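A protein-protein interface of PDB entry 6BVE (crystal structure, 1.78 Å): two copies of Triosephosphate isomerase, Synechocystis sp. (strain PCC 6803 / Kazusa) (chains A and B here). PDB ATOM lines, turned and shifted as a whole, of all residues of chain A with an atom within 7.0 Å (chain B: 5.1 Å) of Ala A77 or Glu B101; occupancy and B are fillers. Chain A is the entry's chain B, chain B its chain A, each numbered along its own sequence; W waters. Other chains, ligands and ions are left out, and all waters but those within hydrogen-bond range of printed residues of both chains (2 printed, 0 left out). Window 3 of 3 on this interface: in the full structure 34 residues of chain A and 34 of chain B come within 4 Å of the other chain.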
ATOM      1  N   HIS A  71     -20.425  32.414  -0.367  1.00  0.00           N
ATOM      2  CA  HIS A  71     -19.885  31.584   0.707  1.00  0.00           C
ATOM      3  C   HIS A  71     -20.665  31.790   2.007  1.00  0.00           C
ATOM      4  O   HIS A  71     -21.450  32.722   2.144  1.00  0.00           O
ATOM      5  CB  HIS A  71     -18.407  31.892   0.925  1.00  0.00           C
ATOM      6  CG  HIS A  71     -17.710  30.883   1.779  1.00  0.00           C
ATOM      7  ND1 HIS A  71     -17.487  31.071   3.131  1.00  0.00           N
ATOM      8  CD2 HIS A  71     -17.211  29.662   1.478  1.00  0.00           C
ATOM      9  CE1 HIS A  71     -16.868  30.009   3.618  1.00  0.00           C
ATOM     10  NE2 HIS A  71     -16.691  29.140   2.634  1.00  0.00           N
ATOM     11  N   GLU A  73     -19.307  32.212   5.153  1.00  0.00           N
ATOM     12  CA  GLU A  73     -18.667  33.062   6.146  1.00  0.00           C
ATOM     13  C   GLU A  73     -18.589  34.492   5.629  1.00  0.00           C
ATOM     14  O   GLU A  73     -18.605  34.734   4.419  1.00  0.00           O
ATOM     15  CB  GLU A  73     -17.263  32.551   6.505  1.00  0.00           C
ATOM     16  CG  GLU A  73     -17.247  31.163   7.214  1.00  0.00           C
ATOM     17  CD  GLU A  73     -17.934  31.144   8.608  1.00  0.00           C
ATOM     18  OE1 GLU A  73     -18.451  32.176   9.092  1.00  0.00           O
ATOM     19  OE2 GLU A  73     -17.947  30.068   9.228  1.00  0.00           O
ATOM     20  N   SER A  75     -16.056  36.558   5.834  1.00  0.00           N
ATOM     21  CA  SER A  75     -14.718  36.753   5.283  1.00  0.00           C
ATOM     22  C   SER A  75     -13.899  35.562   5.763  1.00  0.00           C
ATOM     23  O   SER A  75     -14.307  34.853   6.690  1.00  0.00           O
ATOM     24  CB  SER A  75     -14.077  38.072   5.749  1.00  0.00           C
ATOM     25  OG  SER A  75     -13.820  38.017   7.147  1.00  0.00           O
ATOM     26  N   GLY A  76     -12.736  35.355   5.160  1.00  0.00           N
ATOM     27  CA  GLY A  76     -11.817  34.389   5.734  1.00  0.00           C
ATOM     28  C   GLY A  76     -11.029  33.626   4.679  1.00  0.00           C
ATOM     29  O   GLY A  76     -10.925  34.036   3.515  1.00  0.00           O
ATOM     30  N   ALA A  77     -10.464  32.504   5.135  1.00  0.00           N
ATOM     31  CA  ALA A  77      -9.441  31.770   4.380  1.00  0.00           C
ATOM     32  C   ALA A  77     -10.123  30.767   3.450  1.00  0.00           C
ATOM     33  O   ALA A  77     -10.098  29.546   3.649  1.00  0.00           O
ATOM     34  CB  ALA A  77      -8.471  31.079   5.329  1.00  0.00           C
ATOM     35  N   TYR A  78     -10.778  31.323   2.431  1.00  0.00           N
ATOM     36  CA  TYR A  78     -11.539  30.544   1.460  1.00  0.00           C
ATOM     37  C   TYR A  78     -11.177  31.084   0.082  1.00  0.00           C
ATOM     38  O   TYR A  78     -11.961  31.781  -0.562  1.00  0.00           O
ATOM     39  CB  TYR A  78     -13.027  30.626   1.723  1.00  0.00           C
ATOM     40  CG  TYR A  78     -13.355  30.179   3.107  1.00  0.00           C
ATOM     41  CD1 TYR A  78     -13.452  28.829   3.418  1.00  0.00           C
ATOM     42  CD2 TYR A  78     -13.540  31.115   4.119  1.00  0.00           C
ATOM     43  CE1 TYR A  78     -13.742  28.421   4.720  1.00  0.00           C
ATOM     44  CE2 TYR A  78     -13.840  30.711   5.416  1.00  0.00           C
ATOM     45  CZ  TYR A  78     -13.933  29.374   5.706  1.00  0.00           C
ATOM     46  OH  TYR A  78     -14.226  29.002   7.002  1.00  0.00           O
ATOM     47  N   THR A  79      -9.963  30.772  -0.346  1.00  0.00           N
ATOM     48  CA  THR A  79      -9.468  31.250  -1.630  1.00  0.00           C
ATOM     49  C   THR A  79     -10.458  30.902  -2.738  1.00  0.00           C
ATOM     50  O   THR A  79     -10.934  29.767  -2.819  1.00  0.00           O
ATOM     51  CB  THR A  79      -8.102  30.620  -1.902  1.00  0.00           C
ATOM     52  OG1 THR A  79      -7.166  31.096  -0.925  1.00  0.00           O
ATOM     53  CG2 THR A  79      -7.610  30.968  -3.299  1.00  0.00           C
ATOM     54  N   GLY A  80     -10.778  31.895  -3.582  1.00  0.00           N
ATOM     55  CA  GLY A  80     -11.707  31.736  -4.684  1.00  0.00           C
ATOM     56  C   GLY A  80     -13.168  32.046  -4.377  1.00  0.00           C
ATOM     57  O   GLY A  80     -13.951  32.218  -5.322  1.00  0.00           O
ATOM     58  N   LYS B  14      -7.480  36.045  -0.344  1.00  0.00           N
ATOM     59  CA  LYS B  14      -8.513  35.031  -0.059  1.00  0.00           C
ATOM     60  C   LYS B  14      -9.878  35.725  -0.094  1.00  0.00           C
ATOM     61  O   LYS B  14     -10.101  36.632  -0.912  1.00  0.00           O
ATOM     62  CB  LYS B  14      -8.185  34.305   1.236  1.00  0.00           C
ATOM     63  CG  LYS B  14      -6.812  33.675   1.177  1.00  0.00           C
ATOM     64  CD  LYS B  14      -6.556  32.695   2.320  1.00  0.00           C
ATOM     65  CE  LYS B  14      -5.124  32.164   2.249  1.00  0.00           C
ATOM     66  NZ  LYS B  14      -4.824  31.127   3.314  1.00  0.00           N
ATOM     67  N   HIS B  16     -11.486  38.195   1.234  1.00  0.00           N
ATOM     68  CA  HIS B  16     -11.436  39.451   1.961  1.00  0.00           C
ATOM     69  C   HIS B  16     -11.510  40.585   0.958  1.00  0.00           C
ATOM     70  O   HIS B  16     -10.978  40.471  -0.152  1.00  0.00           O
ATOM     71  CB  HIS B  16     -10.148  39.617   2.754  1.00  0.00           C
ATOM     72  CG  HIS B  16     -10.013  38.684   3.909  1.00  0.00           C
ATOM     73  ND1 HIS B  16     -10.516  38.977   5.162  1.00  0.00           N
ATOM     74  CD2 HIS B  16      -9.412  37.476   4.011  1.00  0.00           C
ATOM     75  CE1 HIS B  16     -10.234  37.979   5.983  1.00  0.00           C
ATOM     76  NE2 HIS B  16      -9.565  37.061   5.312  1.00  0.00           N
ATOM     77  N   HIS B  99      -5.083  26.086  -4.994  1.00  0.00           N
ATOM     78  CA  HIS B  99      -4.857  26.445  -3.604  1.00  0.00           C
ATOM     79  C   HIS B  99      -5.415  25.375  -2.675  1.00  0.00           C
ATOM     80  O   HIS B  99      -6.483  24.814  -2.922  1.00  0.00           O
ATOM     81  CB  HIS B  99      -5.511  27.785  -3.277  1.00  0.00           C
ATOM     82  CG  HIS B  99      -5.000  28.362  -2.005  1.00  0.00           C
ATOM     83  ND1 HIS B  99      -5.515  28.025  -0.772  1.00  0.00           N
ATOM     84  CD2 HIS B  99      -3.956  29.187  -1.767  1.00  0.00           C
ATOM     85  CE1 HIS B  99      -4.830  28.645   0.169  1.00  0.00           C
ATOM     86  NE2 HIS B  99      -3.880  29.358  -0.408  1.00  0.00           N
ATOM     87  N   SER B 100      -4.681  25.117  -1.583  1.00  0.00           N
ATOM     88  CA  SER B 100      -5.067  24.070  -0.639  1.00  0.00           C
ATOM     89  C   SER B 100      -6.519  24.210  -0.197  1.00  0.00           C
ATOM     90  O   SER B 100      -7.214  23.208   0.004  1.00  0.00           O
ATOM     91  CB  SER B 100      -4.139  24.090   0.582  1.00  0.00           C
ATOM     92  OG  SER B 100      -4.595  23.202   1.603  1.00  0.00           O
ATOM     93  N   GLU B 101      -7.008  25.447  -0.064  1.00  0.00           N
ATOM     94  CA  GLU B 101      -8.375  25.628   0.433  1.00  0.00           C
ATOM     95  C   GLU B 101      -9.402  25.127  -0.571  1.00  0.00           C
ATOM     96  O   GLU B 101     -10.457  24.605  -0.181  1.00  0.00           O
ATOM     97  CB  GLU B 101      -8.622  27.098   0.791  1.00  0.00           C
ATOM     98  CG  GLU B 101      -7.950  27.443   2.095  1.00  0.00           C
ATOM     99  CD  GLU B 101      -7.453  28.883   2.182  1.00  0.00           C
ATOM    100  OE1 GLU B 101      -7.875  29.733   1.375  1.00  0.00           O
ATOM    101  OE2 GLU B 101      -6.626  29.155   3.075  1.00  0.00           O
ATOM    102  N   ARG B 102      -9.093  25.221  -1.856  1.00  0.00           N
ATOM    103  CA  ARG B 102      -9.996  24.631  -2.829  1.00  0.00           C
ATOM    104  C   ARG B 102      -9.879  23.114  -2.859  1.00  0.00           C
ATOM    105  O   ARG B 102     -10.872  22.436  -3.142  1.00  0.00           O
ATOM    106  CB  ARG B 102      -9.735  25.256  -4.191  1.00  0.00           C
ATOM    107  CG  ARG B 102      -9.823  26.806  -4.045  1.00  0.00           C
ATOM    108  CD  ARG B 102     -10.510  27.480  -5.164  1.00  0.00           C
ATOM    109  NE  ARG B 102     -11.827  26.948  -5.517  1.00  0.00           N
ATOM    110  CZ  ARG B 102     -12.986  27.429  -5.077  1.00  0.00           C
ATOM    111  NH1 ARG B 102     -13.030  28.412  -4.182  1.00  0.00           N
ATOM    112  NH2 ARG B 102     -14.121  26.900  -5.516  1.00  0.00           N
ATOM    113  N   ARG B 103      -8.694  22.563  -2.566  1.00  0.00           N
ATOM    114  CA  ARG B 103      -8.581  21.104  -2.475  1.00  0.00           C
ATOM    115  C   ARG B 103      -9.256  20.578  -1.210  1.00  0.00           C
ATOM    116  O   ARG B 103      -9.873  19.504  -1.221  1.00  0.00           O
ATOM    117  CB  ARG B 103      -7.113  20.679  -2.506  1.00  0.00           C
ATOM    118  CG  ARG B 103      -6.322  21.209  -3.690  1.00  0.00           C
ATOM    119  CD  ARG B 103      -4.846  20.782  -3.570  1.00  0.00           C
ATOM    120  NE  ARG B 103      -3.945  21.294  -4.602  1.00  0.00           N
ATOM    121  CZ  ARG B 103      -3.430  20.552  -5.583  1.00  0.00           C
ATOM    122  NH1 ARG B 103      -3.783  19.263  -5.706  1.00  0.00           N
ATOM    123  NH2 ARG B 103      -2.566  21.088  -6.439  1.00  0.00           N
ATOM    124  N   GLN B 104      -9.145  21.321  -0.110  1.00  0.00           N
ATOM    125  CA  GLN B 104      -9.742  20.885   1.144  1.00  0.00           C
ATOM    126  C   GLN B 104     -11.263  20.939   1.090  1.00  0.00           C
ATOM    127  O   GLN B 104     -11.945  19.989   1.494  1.00  0.00           O
ATOM    128  CB  GLN B 104      -9.229  21.756   2.281  1.00  0.00           C
ATOM    129  CG  GLN B 104      -7.779  21.543   2.638  1.00  0.00           C
ATOM    130  CD  GLN B 104      -7.397  22.399   3.829  1.00  0.00           C
ATOM    131  OE1 GLN B 104      -8.092  22.384   4.851  1.00  0.00           O
ATOM    132  NE2 GLN B 104      -6.323  23.175   3.694  1.00  0.00           N
ATOM    133  N   TYR B 105     -11.817  22.043   0.606  1.00  0.00           N
ATOM    134  CA  TYR B 105     -13.247  22.285   0.743  1.00  0.00           C
ATOM    135  C   TYR B 105     -14.033  22.106  -0.533  1.00  0.00           C
ATOM    136  O   TYR B 105     -15.224  21.804  -0.465  1.00  0.00           O
ATOM    137  CB  TYR B 105     -13.525  23.717   1.219  1.00  0.00           C
ATOM    138  CG  TYR B 105     -12.800  24.151   2.470  1.00  0.00           C
ATOM    139  CD1 TYR B 105     -12.894  23.426   3.646  1.00  0.00           C
ATOM    140  CD2 TYR B 105     -12.050  25.307   2.478  1.00  0.00           C
ATOM    141  CE1 TYR B 105     -12.232  23.841   4.799  1.00  0.00           C
ATOM    142  CE2 TYR B 105     -11.402  25.736   3.631  1.00  0.00           C
ATOM    143  CZ  TYR B 105     -11.489  25.001   4.778  1.00  0.00           C
ATOM    144  OH  TYR B 105     -10.824  25.449   5.908  1.00  0.00           O
ATOM    145  N   PHE B 106     -13.431  22.356  -1.687  1.00  0.00           N
ATOM    146  CA  PHE B 106     -14.236  22.581  -2.873  1.00  0.00           C
ATOM    147  C   PHE B 106     -13.912  21.597  -3.997  1.00  0.00           C
ATOM    148  O   PHE B 106     -14.112  21.899  -5.173  1.00  0.00           O
ATOM    149  CB  PHE B 106     -14.085  24.045  -3.303  1.00  0.00           C
ATOM    150  CG  PHE B 106     -14.389  25.023  -2.192  1.00  0.00           C
ATOM    151  CD1 PHE B 106     -15.577  24.916  -1.473  1.00  0.00           C
ATOM    152  CD2 PHE B 106     -13.494  26.049  -1.861  1.00  0.00           C
ATOM    153  CE1 PHE B 106     -15.886  25.792  -0.447  1.00  0.00           C
ATOM    154  CE2 PHE B 106     -13.782  26.938  -0.838  1.00  0.00           C
ATOM    155  CZ  PHE B 106     -14.993  26.817  -0.110  1.00  0.00           C
ATOM    156  N   ILE B 173      -0.265  27.141   6.632  1.00  0.00           N
ATOM    157  CA  ILE B 173      -1.203  28.107   6.070  1.00  0.00           C
ATOM    158  C   ILE B 173      -2.123  28.633   7.169  1.00  0.00           C
ATOM    159  O   ILE B 173      -2.927  27.885   7.741  1.00  0.00           O
ATOM    160  CB  ILE B 173      -2.006  27.486   4.924  1.00  0.00           C
ATOM    161  CG1 ILE B 173      -1.058  27.102   3.777  1.00  0.00           C
ATOM    162  CG2 ILE B 173      -3.087  28.452   4.436  1.00  0.00           C
ATOM    163  CD1 ILE B 173      -1.732  26.371   2.639  1.00  0.00           C
HETATM  164  O   HOH W   1      -9.641  27.979   5.787  1.00  0.00           O
HETATM  165  O   HOH W   2      -8.399  34.898   6.101  1.00  0.00           O
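Among the printed residues, pairs that only touch across the chains: Thr A79 with Lys B14 (3.3 Å), Gly A76 with His B16 (3.5 Å), Gly A76 with Lys B14 (3.6 Å), Gly A80 with Arg B102 (3.6 Å), Ala A77 with Lys B14 (3.7 Å), Tyr A78 with Tyr B105 (3.7 Å), Ser A75 with His B16 (3.7 Å) and His A71 with Phe B106 (3.9 Å).
Hydrophobic or aromatic side chains of chain A that line the printed part of chain B: His A71, Ala A77 and Tyr A78.
Printed residues of chain B that touch a printed residue of chain A: Lys B14, His B16, His B99, Glu B101, Arg B102, Tyr B105 and Phe B106.
Among the printed residues, 13 pairs touch across the chains.
Glu A73 touches none of the printed residues of chain B.
Of the printed residues of chain B, Ser A75 touches His B16.
Of the printed residues of chain B, Gly A76 touches Lys B14 and His B16.
Of chain B, only Lys B14 (3.7 Å) and Glu B101 (3.1 Å) come within 4 Å of Ala A77.
Of the printed residues of chain A, His B16 touches Ser A75 (3.7 Å) and Gly A76 (3.5 Å).
Printed residues of chain A within 4 Å of His B99: Thr A79 (3.5 Å).
Ser B100 touches none of the printed residues of chain A.
Printed residues of chain A within 4 Å of Glu B101: Ala A77 (3.1 Å), Tyr A78 (3.5 Å) and Thr A79 (2.8 Å).
Water W2 lies within hydrogen-bond range of NE2 of His B16 (2.6 Å) and N of Ala A77 (3.3 Å).
Water W1 lies within hydrogen-bond range of O of Ala A77 (2.7 Å) and OH of Tyr B105 (2.8 Å).
No position is printed for both chains.
ND1 of His B99 sits at hydrogen-bond distance from OG1 of Thr A79, 3.5 Å away.
N of Tyr A78 is in hydrogen-bond range of OE1 of Glu B101, at 3.5 Å.
The side-chain carboxylate (OE1) of Glu B101 is in hydrogen-bond range of the side-chain hydroxyl (OG1) of Thr A79, at 2.8 Å.
The backbone carbonyl oxygen (O) of Thr A79 sits at hydrogen-bond distance from the guanidinium group (NH1) of Arg B102 (2.8 Å).
O of Ala A77 sits close to OE1 of Glu B101 (3.2 Å).
The side-chain amino group (NZ) of Lys B14 is in salt-bridge range of the side-chain carboxylate (OE2) of Glu B101.
A ring nitrogen (ND1) of His B99 sits close to the backbone NH of Glu B101 (3.1 Å).
A ring nitrogen (ND1) of His A71 lies within hydrogen-bond range of the backbone NH of Glu A73 (3.0 Å).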
